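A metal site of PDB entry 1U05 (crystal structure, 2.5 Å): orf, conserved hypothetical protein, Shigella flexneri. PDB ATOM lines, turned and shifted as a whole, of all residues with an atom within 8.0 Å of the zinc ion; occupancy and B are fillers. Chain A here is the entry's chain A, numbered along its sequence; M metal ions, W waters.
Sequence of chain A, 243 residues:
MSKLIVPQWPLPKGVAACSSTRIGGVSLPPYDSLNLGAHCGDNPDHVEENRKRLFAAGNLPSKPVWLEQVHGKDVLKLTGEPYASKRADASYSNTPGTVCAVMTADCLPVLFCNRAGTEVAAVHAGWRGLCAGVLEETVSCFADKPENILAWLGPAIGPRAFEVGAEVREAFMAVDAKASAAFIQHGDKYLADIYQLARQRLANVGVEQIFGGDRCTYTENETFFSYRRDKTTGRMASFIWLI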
ATOM      1  N   GLN A  69     -18.742 -21.025 -19.481  1.00  0.00           N
ATOM      2  CA  GLN A  69     -17.609 -21.096 -20.389  1.00  0.00           C
ATOM      3  C   GLN A  69     -16.490 -20.161 -19.951  1.00  0.00           C
ATOM      4  O   GLN A  69     -16.661 -18.935 -19.925  1.00  0.00           O
ATOM      5  CB  GLN A  69     -18.065 -20.784 -21.815  1.00  0.00           C
ATOM      6  CG  GLN A  69     -18.528 -22.014 -22.601  1.00  0.00           C
ATOM      7  CD  GLN A  69     -19.682 -21.731 -23.539  1.00  0.00           C
ATOM      8  OE1 GLN A  69     -19.718 -20.695 -24.195  1.00  0.00           O
ATOM      9  NE2 GLN A  69     -20.623 -22.667 -23.611  1.00  0.00           N
ATOM     10  N   VAL A  70     -15.343 -20.737 -19.587  1.00  0.00           N
ATOM     11  CA  VAL A  70     -14.182 -19.949 -19.156  1.00  0.00           C
ATOM     12  C   VAL A  70     -13.027 -20.111 -20.132  1.00  0.00           C
ATOM     13  O   VAL A  70     -11.865 -19.869 -19.776  1.00  0.00           O
ATOM     14  CB  VAL A  70     -13.719 -20.348 -17.730  1.00  0.00           C
ATOM     15  CG1 VAL A  70     -14.858 -20.188 -16.749  1.00  0.00           C
ATOM     16  CG2 VAL A  70     -13.194 -21.769 -17.728  1.00  0.00           C
ATOM     17  N   HIS A  71     -13.344 -20.513 -21.356  1.00  0.00           N
ATOM     18  CA  HIS A  71     -12.342 -20.702 -22.402  1.00  0.00           C
ATOM     19  C   HIS A  71     -11.206 -21.642 -22.028  1.00  0.00           C
ATOM     20  O   HIS A  71     -10.086 -21.507 -22.532  1.00  0.00           O
ATOM     21  CB  HIS A  71     -11.784 -19.353 -22.844  1.00  0.00           C
ATOM     22  CG  HIS A  71     -12.735 -18.557 -23.690  1.00  0.00           C
ATOM     23  ND1 HIS A  71     -13.892 -18.017 -23.192  1.00  0.00           N
ATOM     24  CD2 HIS A  71     -12.707 -18.240 -25.003  1.00  0.00           C
ATOM     25  CE1 HIS A  71     -14.550 -17.400 -24.157  1.00  0.00           C
ATOM     26  NE2 HIS A  71     -13.846 -17.520 -25.272  1.00  0.00           N
ATOM     27  N   ASP A  89     -15.875 -25.831 -20.667  1.00  0.00           N
ATOM     28  CA  ASP A  89     -16.120 -25.426 -22.045  1.00  0.00           C
ATOM     29  C   ASP A  89     -16.520 -26.587 -22.939  1.00  0.00           C
ATOM     30  O   ASP A  89     -16.347 -26.558 -24.148  1.00  0.00           O
ATOM     31  CB  ASP A  89     -14.871 -24.733 -22.609  1.00  0.00           C
ATOM     32  CG  ASP A  89     -14.608 -23.406 -21.940  1.00  0.00           C
ATOM     33  OD1 ASP A  89     -15.055 -22.355 -22.486  1.00  0.00           O
ATOM     34  OD2 ASP A  89     -13.970 -23.399 -20.865  1.00  0.00           O
ATOM     35  N   MET A 103     -22.206 -22.080 -26.122  1.00  0.00           N
ATOM     36  CA  MET A 103     -22.528 -20.723 -26.562  1.00  0.00           C
ATOM     37  C   MET A 103     -21.355 -20.019 -27.248  1.00  0.00           C
ATOM     38  O   MET A 103     -20.273 -19.852 -26.653  1.00  0.00           O
ATOM     39  CB  MET A 103     -22.988 -19.918 -25.350  1.00  0.00           C
ATOM     40  CG  MET A 103     -23.425 -18.517 -25.676  1.00  0.00           C
ATOM     41  SD  MET A 103     -24.660 -18.029 -24.497  1.00  0.00           S
ATOM     42  CE  MET A 103     -26.114 -18.718 -25.268  1.00  0.00           C
ATOM     43  N   THR A 104     -21.553 -19.585 -28.490  1.00  0.00           N
ATOM     44  CA  THR A 104     -20.466 -18.933 -29.217  1.00  0.00           C
ATOM     45  C   THR A 104     -20.830 -17.711 -30.047  1.00  0.00           C
ATOM     46  O   THR A 104     -22.010 -17.418 -30.260  1.00  0.00           O
ATOM     47  CB  THR A 104     -19.775 -19.931 -30.183  1.00  0.00           C
ATOM     48  OG1 THR A 104     -20.713 -20.334 -31.182  1.00  0.00           O
ATOM     49  CG2 THR A 104     -19.262 -21.160 -29.422  1.00  0.00           C
ATOM     50  N   ALA A 105     -19.790 -17.026 -30.514  1.00  0.00           N
ATOM     51  CA  ALA A 105     -19.897 -15.849 -31.365  1.00  0.00           C
ATOM     52  C   ALA A 105     -18.491 -15.572 -31.955  1.00  0.00           C
ATOM     53  O   ALA A 105     -17.939 -14.479 -31.799  1.00  0.00           O
ATOM     54  CB  ALA A 105     -20.393 -14.651 -30.556  1.00  0.00           C
ATOM     55  N   ASP A 106     -17.951 -16.606 -32.614  1.00  0.00           N
ATOM     56  CA  ASP A 106     -16.643 -16.642 -33.267  1.00  0.00           C
ATOM     57  C   ASP A 106     -15.875 -17.921 -32.906  1.00  0.00           C
ATOM     58  O   ASP A 106     -15.315 -18.594 -33.778  1.00  0.00           O
ATOM     59  CB  ASP A 106     -15.751 -15.438 -32.901  1.00  0.00           C
ATOM     60  CG  ASP A 106     -15.995 -14.235 -33.791  1.00  0.00           C
ATOM     61  OD1 ASP A 106     -16.294 -14.412 -34.988  1.00  0.00           O
ATOM     62  OD2 ASP A 106     -15.854 -13.097 -33.302  1.00  0.00           O
ATOM     63  N   CYS A 107     -15.839 -18.244 -31.623  1.00  0.00           N
ATOM     64  CA  CYS A 107     -15.143 -19.434 -31.189  1.00  0.00           C
ATOM     65  C   CYS A 107     -15.730 -20.656 -31.852  1.00  0.00           C
ATOM     66  O   CYS A 107     -16.888 -20.668 -32.270  1.00  0.00           O
ATOM     67  CB  CYS A 107     -15.165 -19.543 -29.667  1.00  0.00           C
ATOM     68  SG  CYS A 107     -14.063 -18.334 -28.882  1.00  0.00           S
ATOM     69  N   LEU A 108     -14.922 -21.699 -31.953  1.00  0.00           N
ATOM     70  CA  LEU A 108     -15.337 -22.921 -32.617  1.00  0.00           C
ATOM     71  C   LEU A 108     -16.314 -23.816 -31.885  1.00  0.00           C
ATOM     72  O   LEU A 108     -16.025 -24.293 -30.811  1.00  0.00           O
ATOM     73  CB  LEU A 108     -14.107 -23.735 -32.986  1.00  0.00           C
ATOM     74  CG  LEU A 108     -14.361 -25.053 -33.698  1.00  0.00           C
ATOM     75  CD1 LEU A 108     -15.085 -24.786 -35.014  1.00  0.00           C
ATOM     76  CD2 LEU A 108     -13.039 -25.795 -33.920  1.00  0.00           C
ATOM     77  N   HIS A 124     -17.037 -25.823 -26.901  1.00  0.00           N
ATOM     78  CA  HIS A 124     -16.797 -24.433 -27.250  1.00  0.00           C
ATOM     79  C   HIS A 124     -15.274 -24.411 -27.280  1.00  0.00           C
ATOM     80  O   HIS A 124     -14.628 -24.567 -26.245  1.00  0.00           O
ATOM     81  CB  HIS A 124     -17.319 -23.506 -26.155  1.00  0.00           C
ATOM     82  CG  HIS A 124     -16.648 -22.163 -26.127  1.00  0.00           C
ATOM     83  ND1 HIS A 124     -15.761 -21.796 -25.136  1.00  0.00           N
ATOM     84  CD2 HIS A 124     -16.692 -21.128 -26.990  1.00  0.00           C
ATOM     85  CE1 HIS A 124     -15.294 -20.589 -25.395  1.00  0.00           C
ATOM     86  NE2 HIS A 124     -15.840 -20.163 -26.509  1.00  0.00           N
ATOM     87  N   ALA A 125     -14.695 -24.226 -28.463  1.00  0.00           N
ATOM     88  CA  ALA A 125     -13.246 -24.248 -28.570  1.00  0.00           C
ATOM     89  C   ALA A 125     -12.577 -22.987 -29.076  1.00  0.00           C
ATOM     90  O   ALA A 125     -12.433 -22.796 -30.291  1.00  0.00           O
ATOM     91  CB  ALA A 125     -12.820 -25.426 -29.439  1.00  0.00           C
ATOM     92  N   GLY A 126     -12.168 -22.129 -28.151  1.00  0.00           N
ATOM     93  CA  GLY A 126     -11.452 -20.923 -28.540  1.00  0.00           C
ATOM     94  C   GLY A 126     -10.040 -21.416 -28.797  1.00  0.00           C
ATOM     95  O   GLY A 126      -9.757 -22.593 -28.559  1.00  0.00           O
ATOM     96  N   TRP A 127      -9.133 -20.552 -29.248  1.00  0.00           N
ATOM     97  CA  TRP A 127      -7.790 -21.029 -29.514  1.00  0.00           C
ATOM     98  C   TRP A 127      -7.101 -21.629 -28.293  1.00  0.00           C
ATOM     99  O   TRP A 127      -6.534 -22.714 -28.387  1.00  0.00           O
ATOM    100  CB  TRP A 127      -6.901 -19.958 -30.159  1.00  0.00           C
ATOM    101  CG  TRP A 127      -6.418 -18.835 -29.274  1.00  0.00           C
ATOM    102  CD1 TRP A 127      -6.992 -17.588 -29.141  1.00  0.00           C
ATOM    103  CD2 TRP A 127      -5.213 -18.801 -28.510  1.00  0.00           C
ATOM    104  NE1 TRP A 127      -6.201 -16.792 -28.331  1.00  0.00           N
ATOM    105  CE2 TRP A 127      -5.103 -17.507 -27.934  1.00  0.00           C
ATOM    106  CE3 TRP A 127      -4.195 -19.741 -28.246  1.00  0.00           C
ATOM    107  CZ2 TRP A 127      -4.025 -17.132 -27.118  1.00  0.00           C
ATOM    108  CZ3 TRP A 127      -3.131 -19.364 -27.426  1.00  0.00           C
ATOM    109  CH2 TRP A 127      -3.053 -18.071 -26.881  1.00  0.00           C
ATOM    110  N   TYR A 227     -17.964 -11.551 -32.261  1.00  0.00           N
ATOM    111  CA  TYR A 227     -17.323 -10.749 -31.225  1.00  0.00           C
ATOM    112  C   TYR A 227     -16.177  -9.941 -31.819  1.00  0.00           C
ATOM    113  O   TYR A 227     -15.939  -8.802 -31.424  1.00  0.00           O
ATOM    114  CB  TYR A 227     -16.785 -11.645 -30.124  1.00  0.00           C
ATOM    115  CG  TYR A 227     -16.186 -10.903 -28.965  1.00  0.00           C
ATOM    116  CD1 TYR A 227     -16.995 -10.222 -28.057  1.00  0.00           C
ATOM    117  CD2 TYR A 227     -14.799 -10.863 -28.773  1.00  0.00           C
ATOM    118  CE1 TYR A 227     -16.450  -9.533 -26.981  1.00  0.00           C
ATOM    119  CE2 TYR A 227     -14.246 -10.168 -27.698  1.00  0.00           C
ATOM    120  CZ  TYR A 227     -15.078  -9.512 -26.807  1.00  0.00           C
ATOM    121  OH  TYR A 227     -14.545  -8.813 -25.747  1.00  0.00           O
ATOM    122  N   ARG A 235     -25.254 -13.805 -29.231  1.00  0.00           N
ATOM    123  CA  ARG A 235     -24.563 -15.078 -29.182  1.00  0.00           C
ATOM    124  C   ARG A 235     -25.372 -16.151 -29.866  1.00  0.00           C
ATOM    125  O   ARG A 235     -26.598 -16.125 -29.808  1.00  0.00           O
ATOM    126  CB  ARG A 235     -24.361 -15.504 -27.719  1.00  0.00           C
ATOM    127  CG  ARG A 235     -23.432 -14.626 -26.881  1.00  0.00           C
ATOM    128  CD  ARG A 235     -22.000 -14.737 -27.381  1.00  0.00           C
ATOM    129  NE  ARG A 235     -21.076 -13.956 -26.572  1.00  0.00           N
ATOM    130  CZ  ARG A 235     -20.857 -12.661 -26.724  1.00  0.00           C
ATOM    131  NH1 ARG A 235     -21.503 -11.975 -27.675  1.00  0.00           N
ATOM    132  NH2 ARG A 235     -19.997 -12.044 -25.921  1.00  0.00           N
HETATM  133 ZN    ZN M   1     -15.327 -18.094 -26.950  1.00  0.00          ZN
HETATM  134  O   HOH W   1     -17.027 -16.814 -27.914  1.00  0.00           O
HETATM  135  O   HOH W   2     -14.958 -15.321 -28.970  1.00  0.00           O
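The zinc ion is bound by a ring nitrogen (NE2) of His 124 (2.2 Å), a ring nitrogen (NE2) of His 71 (2.3 Å), the side-chain sulfur (SG) of Cys 107 (2.3 Å) and water W1 (2.3 Å).
The zinc ion has four donor atoms within binding distance.
The nearest printed residue that does not touch the zinc ion is Gly 126 (5.1 Å).
OD1 of Asp 89 sits at hydrogen-bond distance from N of His 71 (2.8 Å).
A ring nitrogen (ND1) of His 124 lies within hydrogen-bond range of the side-chain carboxylate (OD1) of Asp 89 (2.8 Å).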
